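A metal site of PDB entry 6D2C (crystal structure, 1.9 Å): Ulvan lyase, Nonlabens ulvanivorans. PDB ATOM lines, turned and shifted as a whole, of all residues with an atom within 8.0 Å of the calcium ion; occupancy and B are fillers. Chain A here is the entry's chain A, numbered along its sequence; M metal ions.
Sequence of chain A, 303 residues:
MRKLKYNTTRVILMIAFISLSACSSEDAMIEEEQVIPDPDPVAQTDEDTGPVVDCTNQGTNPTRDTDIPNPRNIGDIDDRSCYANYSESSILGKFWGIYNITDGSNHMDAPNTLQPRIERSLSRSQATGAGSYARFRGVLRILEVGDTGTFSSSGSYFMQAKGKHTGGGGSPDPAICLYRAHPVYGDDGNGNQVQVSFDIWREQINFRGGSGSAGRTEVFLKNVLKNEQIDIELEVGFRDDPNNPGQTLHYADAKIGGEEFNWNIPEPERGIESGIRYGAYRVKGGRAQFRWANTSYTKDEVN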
ATOM      1  N   THR A  56       7.127  20.382  -6.458  1.00  0.00           N
ATOM      2  CA  THR A  56       7.289  20.142  -5.024  1.00  0.00           C
ATOM      3  C   THR A  56       7.052  18.661  -4.768  1.00  0.00           C
ATOM      4  O   THR A  56       6.387  17.979  -5.558  1.00  0.00           O
ATOM      5  CB  THR A  56       6.359  20.975  -4.134  1.00  0.00           C
ATOM      6  OG1 THR A  56       5.021  20.491  -4.220  1.00  0.00           O
ATOM      7  CG2 THR A  56       6.406  22.425  -4.530  1.00  0.00           C
ATOM      8  N   ASN A  57       7.643  18.161  -3.673  1.00  0.00           N
ATOM      9  CA  ASN A  57       7.389  16.766  -3.300  1.00  0.00           C
ATOM     10  C   ASN A  57       5.908  16.478  -3.272  1.00  0.00           C
ATOM     11  O   ASN A  57       5.449  15.478  -3.849  1.00  0.00           O
ATOM     12  CB  ASN A  57       7.974  16.456  -1.922  1.00  0.00           C
ATOM     13  CG  ASN A  57       9.494  16.317  -1.931  1.00  0.00           C
ATOM     14  OD1 ASN A  57      10.128  16.472  -2.954  1.00  0.00           O
ATOM     15  ND2 ASN A  57      10.067  16.068  -0.763  1.00  0.00           N
ATOM     16  N   GLN A  58       5.152  17.315  -2.538  1.00  0.00           N
ATOM     17  CA  GLN A  58       3.744  17.052  -2.302  1.00  0.00           C
ATOM     18  C   GLN A  58       2.920  17.135  -3.572  1.00  0.00           C
ATOM     19  O   GLN A  58       1.786  16.630  -3.600  1.00  0.00           O
ATOM     20  CB  GLN A  58       3.142  18.006  -1.272  1.00  0.00           C
ATOM     21  CG  GLN A  58       3.324  19.497  -1.565  1.00  0.00           C
ATOM     22  CD  GLN A  58       4.640  20.066  -1.040  1.00  0.00           C
ATOM     23  OE1 GLN A  58       5.640  19.347  -0.841  1.00  0.00           O
ATOM     24  NE2 GLN A  58       4.658  21.358  -0.822  1.00  0.00           N
ATOM     25  N   GLY A  59       3.438  17.776  -4.612  1.00  0.00           N
ATOM     26  CA  GLY A  59       2.723  17.775  -5.880  1.00  0.00           C
ATOM     27  C   GLY A  59       3.223  16.755  -6.887  1.00  0.00           C
ATOM     28  O   GLY A  59       2.703  16.691  -8.016  1.00  0.00           O
ATOM     29  N   THR A  60       4.236  15.951  -6.549  1.00  0.00           N
ATOM     30  CA  THR A  60       4.831  15.053  -7.548  1.00  0.00           C
ATOM     31  C   THR A  60       4.084  13.727  -7.510  1.00  0.00           C
ATOM     32  O   THR A  60       4.590  12.711  -7.054  1.00  0.00           O
ATOM     33  CB  THR A  60       6.333  14.880  -7.298  1.00  0.00           C
ATOM     34  OG1 THR A  60       6.956  16.161  -7.353  1.00  0.00           O
ATOM     35  CG2 THR A  60       7.008  13.974  -8.402  1.00  0.00           C
ATOM     36  N   ASN A  61       2.882  13.723  -8.094  1.00  0.00           N
ATOM     37  CA  ASN A  61       2.084  12.494  -8.127  1.00  0.00           C
ATOM     38  C   ASN A  61       2.680  11.489  -9.109  1.00  0.00           C
ATOM     39  O   ASN A  61       3.174  11.876 -10.184  1.00  0.00           O
ATOM     40  CB  ASN A  61       0.643  12.837  -8.567  1.00  0.00           C
ATOM     41  CG  ASN A  61       0.622  13.686  -9.839  1.00  0.00           C
ATOM     42  OD1 ASN A  61       1.157  14.813  -9.876  1.00  0.00           O
ATOM     43  ND2 ASN A  61      -0.053  13.162 -10.887  1.00  0.00           N
ATOM     44  N   PRO A  62       2.591  10.190  -8.825  1.00  0.00           N
ATOM     45  CA  PRO A  62       3.148   9.184  -9.736  1.00  0.00           C
ATOM     46  C   PRO A  62       2.227   8.797 -10.902  1.00  0.00           C
ATOM     47  O   PRO A  62       2.727   8.256 -11.891  1.00  0.00           O
ATOM     48  CB  PRO A  62       3.364   7.959  -8.816  1.00  0.00           C
ATOM     49  CG  PRO A  62       2.252   8.076  -7.812  1.00  0.00           C
ATOM     50  CD  PRO A  62       2.059   9.589  -7.570  1.00  0.00           C
ATOM     51  N   THR A  63       0.929   9.059 -10.823  1.00  0.00           N
ATOM     52  CA  THR A  63      -0.018   8.705 -11.877  1.00  0.00           C
ATOM     53  C   THR A  63      -0.983   9.876 -12.054  1.00  0.00           C
ATOM     54  O   THR A  63      -1.243  10.599 -11.106  1.00  0.00           O
ATOM     55  CB  THR A  63      -0.853   7.431 -11.532  1.00  0.00           C
ATOM     56  OG1 THR A  63      -1.567   7.667 -10.315  1.00  0.00           O
ATOM     57  CG2 THR A  63       0.023   6.225 -11.367  1.00  0.00           C
ATOM     58  N   ARG A  64      -1.563  10.024 -13.259  1.00  0.00           N
ATOM     59  CA  ARG A  64      -2.500  11.130 -13.484  1.00  0.00           C
ATOM     60  C   ARG A  64      -3.746  11.002 -12.630  1.00  0.00           C
ATOM     61  O   ARG A  64      -4.411  12.003 -12.348  1.00  0.00           O
ATOM     62  CB  ARG A  64      -2.908  11.184 -14.985  1.00  0.00           C
ATOM     63  CG  ARG A  64      -1.697  11.491 -15.906  1.00  0.00           C
ATOM     64  CD  ARG A  64      -2.062  11.623 -17.333  1.00  0.00           C
ATOM     65  NE  ARG A  64      -2.663  10.364 -17.854  1.00  0.00           N
ATOM     66  CZ  ARG A  64      -3.940  10.205 -18.137  1.00  0.00           C
ATOM     67  NH1 ARG A  64      -4.805  11.195 -17.941  1.00  0.00           N
ATOM     68  NH2 ARG A  64      -4.363   9.040 -18.629  1.00  0.00           N
ATOM     69  N   THR A  66      -4.069  10.422  -9.552  1.00  0.00           N
ATOM     70  CA  THR A  66      -3.872  10.635  -8.118  1.00  0.00           C
ATOM     71  C   THR A  66      -4.857  11.644  -7.572  1.00  0.00           C
ATOM     72  O   THR A  66      -4.853  12.803  -8.008  1.00  0.00           O
ATOM     73  CB  THR A  66      -2.443  11.095  -7.895  1.00  0.00           C
ATOM     74  OG1 THR A  66      -1.579  10.009  -8.253  1.00  0.00           O
ATOM     75  CG2 THR A  66      -2.232  11.521  -6.422  1.00  0.00           C
ATOM     76  N   ILE A  77     -10.076  12.971 -11.699  1.00  0.00           N
ATOM     77  CA  ILE A  77      -8.878  13.828 -11.689  1.00  0.00           C
ATOM     78  C   ILE A  77      -7.945  13.425 -12.803  1.00  0.00           C
ATOM     79  O   ILE A  77      -7.845  12.256 -13.187  1.00  0.00           O
ATOM     80  CB  ILE A  77      -8.168  13.743 -10.319  1.00  0.00           C
ATOM     81  CG1 ILE A  77      -7.155  14.874 -10.155  1.00  0.00           C
ATOM     82  CG2 ILE A  77      -7.387  12.415 -10.207  1.00  0.00           C
ATOM     83  CD1 ILE A  77      -7.775  16.239 -10.074  1.00  0.00           C
ATOM     84  N   ASP A  78      -7.214  14.402 -13.328  1.00  0.00           N
ATOM     85  CA  ASP A  78      -6.221  14.207 -14.399  1.00  0.00           C
ATOM     86  C   ASP A  78      -5.105  15.204 -14.041  1.00  0.00           C
ATOM     87  O   ASP A  78      -5.154  16.377 -14.438  1.00  0.00           O
ATOM     88  CB  ASP A  78      -6.847  14.490 -15.765  1.00  0.00           C
ATOM     89  CG  ASP A  78      -5.915  14.207 -16.932  1.00  0.00           C
ATOM     90  OD1 ASP A  78      -4.739  13.831 -16.746  1.00  0.00           O
ATOM     91  OD2 ASP A  78      -6.354  14.423 -18.087  1.00  0.00           O
ATOM     92  N   ASP A  79      -4.139  14.733 -13.231  1.00  0.00           N
ATOM     93  CA  ASP A  79      -3.114  15.577 -12.600  1.00  0.00           C
ATOM     94  C   ASP A  79      -1.825  15.423 -13.397  1.00  0.00           C
ATOM     95  O   ASP A  79      -1.165  14.373 -13.345  1.00  0.00           O
ATOM     96  CB  ASP A  79      -2.959  15.166 -11.118  1.00  0.00           C
ATOM     97  CG  ASP A  79      -1.819  15.919 -10.408  1.00  0.00           C
ATOM     98  OD1 ASP A  79      -0.985  16.592 -11.081  1.00  0.00           O
ATOM     99  OD2 ASP A  79      -1.776  15.838  -9.146  1.00  0.00           O
ATOM    100  N   ARG A  80      -1.468  16.452 -14.156  1.00  0.00           N
ATOM    101  CA  ARG A  80      -0.241  16.472 -14.932  1.00  0.00           C
ATOM    102  C   ARG A  80       0.595  17.693 -14.579  1.00  0.00           C
ATOM    103  O   ARG A  80       1.041  18.444 -15.455  1.00  0.00           O
ATOM    104  CB  ARG A  80      -0.530  16.461 -16.439  1.00  0.00           C
ATOM    105  CG  ARG A  80      -1.629  15.474 -16.850  1.00  0.00           C
ATOM    106  CD  ARG A  80      -1.681  15.391 -18.418  1.00  0.00           C
ATOM    107  NE  ARG A  80      -2.991  14.888 -18.831  1.00  0.00           N
ATOM    108  CZ  ARG A  80      -3.371  14.735 -20.100  1.00  0.00           C
ATOM    109  NH1 ARG A  80      -2.516  15.024 -21.089  1.00  0.00           N
ATOM    110  NH2 ARG A  80      -4.599  14.311 -20.366  1.00  0.00           N
ATOM    111  N   SER A  81       0.808  17.903 -13.261  1.00  0.00           N
ATOM    112  CA  SER A  81       1.667  18.973 -12.757  1.00  0.00           C
ATOM    113  C   SER A  81       2.361  18.446 -11.508  1.00  0.00           C
ATOM    114  O   SER A  81       1.688  17.965 -10.582  1.00  0.00           O
ATOM    115  CB  SER A  81       0.871  20.224 -12.346  1.00  0.00           C
ATOM    116  OG  SER A  81       1.773  21.238 -11.855  1.00  0.00           O
ATOM    117  N   CYS A  82       3.680  18.546 -11.479  1.00  0.00           N
ATOM    118  CA  CYS A  82       4.377  18.116 -10.278  1.00  0.00           C
ATOM    119  C   CYS A  82       4.463  19.269  -9.267  1.00  0.00           C
ATOM    120  O   CYS A  82       5.063  19.098  -8.196  1.00  0.00           O
ATOM    121  CB  CYS A  82       5.775  17.511 -10.626  1.00  0.00           C
ATOM    122  SG  CYS A  82       6.782  18.714 -11.526  1.00  0.00           S
ATOM    123  N   TYR A  83       3.864  20.428  -9.581  1.00  0.00           N
ATOM    124  CA  TYR A  83       3.874  21.555  -8.644  1.00  0.00           C
ATOM    125  C   TYR A  83       2.947  21.292  -7.469  1.00  0.00           C
ATOM    126  O   TYR A  83       3.281  21.629  -6.307  1.00  0.00           O
ATOM    127  CB  TYR A  83       3.493  22.866  -9.358  1.00  0.00           C
ATOM    128  CG  TYR A  83       3.465  24.051  -8.399  1.00  0.00           C
ATOM    129  CD1 TYR A  83       4.652  24.535  -7.825  1.00  0.00           C
ATOM    130  CD2 TYR A  83       2.264  24.630  -8.011  1.00  0.00           C
ATOM    131  CE1 TYR A  83       4.624  25.601  -6.911  1.00  0.00           C
ATOM    132  CE2 TYR A  83       2.217  25.707  -7.093  1.00  0.00           C
ATOM    133  CZ  TYR A  83       3.426  26.193  -6.550  1.00  0.00           C
ATOM    134  OH  TYR A  83       3.386  27.251  -5.641  1.00  0.00           O
ATOM    135  N   ALA A  84       1.771  20.734  -7.731  1.00  0.00           N
ATOM    136  CA  ALA A  84       0.774  20.544  -6.691  1.00  0.00           C
ATOM    137  C   ALA A  84      -0.069  19.343  -7.057  1.00  0.00           C
ATOM    138  O   ALA A  84      -0.044  18.883  -8.192  1.00  0.00           O
ATOM    139  CB  ALA A  84      -0.105  21.811  -6.528  1.00  0.00           C
ATOM    140  N   ASN A  85      -0.799  18.824  -6.089  1.00  0.00           N
ATOM    141  CA  ASN A  85      -1.860  17.876  -6.337  1.00  0.00           C
ATOM    142  C   ASN A  85      -3.168  18.564  -5.991  1.00  0.00           C
ATOM    143  O   ASN A  85      -3.192  19.559  -5.271  1.00  0.00           O
ATOM    144  CB  ASN A  85      -1.725  16.621  -5.455  1.00  0.00           C
ATOM    145  CG  ASN A  85      -0.616  15.718  -5.867  1.00  0.00           C
ATOM    146  OD1 ASN A  85       0.093  16.007  -6.811  1.00  0.00           O
ATOM    147  ND2 ASN A  85      -0.451  14.613  -5.135  1.00  0.00           N
ATOM    148  N   TYR A  86      -4.266  17.960  -6.425  1.00  0.00           N
ATOM    149  CA  TYR A  86      -5.564  18.429  -5.938  1.00  0.00           C
ATOM    150  C   TYR A  86      -5.599  18.371  -4.409  1.00  0.00           C
ATOM    151  O   TYR A  86      -5.168  17.380  -3.798  1.00  0.00           O
ATOM    152  CB  TYR A  86      -6.688  17.579  -6.518  1.00  0.00           C
ATOM    153  CG  TYR A  86      -8.057  17.942  -5.998  1.00  0.00           C
ATOM    154  CD1 TYR A  86      -8.818  18.908  -6.641  1.00  0.00           C
ATOM    155  CD2 TYR A  86      -8.580  17.310  -4.860  1.00  0.00           C
ATOM    156  CE1 TYR A  86     -10.113  19.235  -6.172  1.00  0.00           C
ATOM    157  CE2 TYR A  86      -9.862  17.609  -4.378  1.00  0.00           C
ATOM    158  CZ  TYR A  86     -10.610  18.572  -5.047  1.00  0.00           C
ATOM    159  OH  TYR A  86     -11.858  18.870  -4.600  1.00  0.00           O
ATOM    160  N   ASN A 100      -3.513  24.412  -8.718  1.00  0.00           N
ATOM    161  CA  ASN A 100      -2.344  25.273  -8.897  1.00  0.00           C
ATOM    162  C   ASN A 100      -1.367  24.590  -9.812  1.00  0.00           C
ATOM    163  O   ASN A 100      -1.064  23.416  -9.600  1.00  0.00           O
ATOM    164  CB  ASN A 100      -1.627  25.539  -7.555  1.00  0.00           C
ATOM    165  CG  ASN A 100      -2.503  26.242  -6.530  1.00  0.00           C
ATOM    166  OD1 ASN A 100      -3.440  26.915  -6.907  1.00  0.00           O
ATOM    167  ND2 ASN A 100      -2.142  26.130  -5.228  1.00  0.00           N
ATOM    168  N   ILE A 101      -0.843  25.320 -10.810  1.00  0.00           N
ATOM    169  CA  ILE A 101       0.153  24.745 -11.705  1.00  0.00           C
ATOM    170  C   ILE A 101       1.185  25.814 -12.029  1.00  0.00           C
ATOM    171  O   ILE A 101       0.939  27.016 -11.917  1.00  0.00           O
ATOM    172  CB  ILE A 101      -0.501  24.210 -13.013  1.00  0.00           C
ATOM    173  CG1 ILE A 101      -1.244  25.355 -13.698  1.00  0.00           C
ATOM    174  CG2 ILE A 101      -1.515  23.058 -12.730  1.00  0.00           C
ATOM    175  CD1 ILE A 101      -1.858  24.893 -15.084  1.00  0.00           C
ATOM    176  N   SER A 105       6.044  22.371 -15.185  1.00  0.00           N
ATOM    177  CA  SER A 105       5.747  21.360 -14.178  1.00  0.00           C
ATOM    178  C   SER A 105       5.088  20.110 -14.745  1.00  0.00           C
ATOM    179  O   SER A 105       4.573  19.289 -13.980  1.00  0.00           O
ATOM    180  CB  SER A 105       4.866  21.928 -13.060  1.00  0.00           C
ATOM    181  OG  SER A 105       3.561  22.336 -13.558  1.00  0.00           O
ATOM    182  N   HIS A 107       5.134  16.690 -15.591  1.00  0.00           N
ATOM    183  CA  HIS A 107       5.939  15.473 -15.495  1.00  0.00           C
ATOM    184  C   HIS A 107       5.213  14.215 -15.979  1.00  0.00           C
ATOM    185  O   HIS A 107       5.749  13.121 -15.845  1.00  0.00           O
ATOM    186  CB  HIS A 107       6.385  15.263 -14.035  1.00  0.00           C
ATOM    187  CG  HIS A 107       5.246  15.003 -13.098  1.00  0.00           C
ATOM    188  ND1 HIS A 107       4.065  15.698 -13.178  1.00  0.00           N
ATOM    189  CD2 HIS A 107       5.074  14.073 -12.128  1.00  0.00           C
ATOM    190  CE1 HIS A 107       3.199  15.234 -12.294  1.00  0.00           C
ATOM    191  NE2 HIS A 107       3.798  14.270 -11.611  1.00  0.00           N
ATOM    192  N   MET A 108       4.016  14.358 -16.570  1.00  0.00           N
ATOM    193  CA  MET A 108       3.180  13.221 -16.944  1.00  0.00           C
ATOM    194  C   MET A 108       3.216  13.040 -18.466  1.00  0.00           C
ATOM    195  O   MET A 108       3.468  11.957 -18.975  1.00  0.00           O
ATOM    196  CB  MET A 108       1.755  13.391 -16.396  1.00  0.00           C
ATOM    197  CG  MET A 108       1.691  13.148 -14.874  1.00  0.00           C
ATOM    198  SD  MET A 108       1.880  11.206 -14.440  1.00  0.00           S
ATOM    199  CE  MET A 108       3.689  11.311 -13.642  1.00  0.00           C
ATOM    200  N   ARG A 117      -1.246  20.596 -16.437  1.00  0.00           N
ATOM    201  CA  ARG A 117      -2.656  20.786 -16.098  1.00  0.00           C
ATOM    202  C   ARG A 117      -2.957  20.014 -14.821  1.00  0.00           C
ATOM    203  O   ARG A 117      -2.287  19.057 -14.498  1.00  0.00           O
ATOM    204  CB  ARG A 117      -3.614  20.280 -17.185  1.00  0.00           C
ATOM    205  CG  ARG A 117      -3.738  18.716 -17.204  1.00  0.00           C
ATOM    206  CD  ARG A 117      -4.784  18.235 -18.374  1.00  0.00           C
ATOM    207  NE  ARG A 117      -4.120  18.277 -19.688  1.00  0.00           N
ATOM    208  CZ  ARG A 117      -4.733  18.523 -20.862  1.00  0.00           C
ATOM    209  NH1 ARG A 117      -6.019  18.828 -20.877  1.00  0.00           N
ATOM    210  NH2 ARG A 117      -4.053  18.468 -22.025  1.00  0.00           N
ATOM    211  N   ILE A 118      -4.011  20.417 -14.113  1.00  0.00           N
ATOM    212  CA  ILE A 118      -4.713  19.522 -13.201  1.00  0.00           C
ATOM    213  C   ILE A 118      -6.173  19.782 -13.512  1.00  0.00           C
ATOM    214  O   ILE A 118      -6.655  20.879 -13.237  1.00  0.00           O
ATOM    215  CB  ILE A 118      -4.426  19.807 -11.709  1.00  0.00           C
ATOM    216  CG1 ILE A 118      -2.907  19.753 -11.408  1.00  0.00           C
ATOM    217  CG2 ILE A 118      -5.271  18.854 -10.793  1.00  0.00           C
ATOM    218  CD1 ILE A 118      -2.489  20.290 -10.000  1.00  0.00           C
HETATM  219 CA    CA M   1       0.486  16.831  -9.074  1.00  0.00          CA
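The side-chain hydroxyl (OG) of Ser 81 lies within hydrogen-bond range of the side-chain hydroxyl (OG) of Ser 105 (2.7 Å).
OG of Ser 81 sits close to N of Tyr 83 (3.2 Å).
ND2 of Asn 85 lies within hydrogen-bond range of O of Gln 58 (3.4 Å).
O of Arg 64 lies within hydrogen-bond range of N of Asp 79, 2.9 Å away.
The backbone carbonyl oxygen of Asn 61 is in hydrogen-bond range of a ring nitrogen (NE2) of His 107, 2.9 Å away.
The backbone NH (N) of Gly 59 lies within hydrogen-bond range of the side-chain hydroxyl (OG1) of Thr 56, at 3.2 Å.
The side-chain amide nitrogen (ND2) of Asn 61 sits at hydrogen-bond distance from the backbone carbonyl oxygen (O) of Thr 63 (2.8 Å).
Six residues have an atom within 4 Å of the calcium ion: Gly 59, Asn 61, Asp 79, Ser 81, Ala 84 and Asn 85.
The calcium ion is bound by O of Ser 81, OD1 of Asn 61, O of Ala 84, OD1 of Asn 85, O of Gly 59, OD2 of Asp 79 and OD1 of Asp 79.
The calcium ion has seven donor atoms within binding distance.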
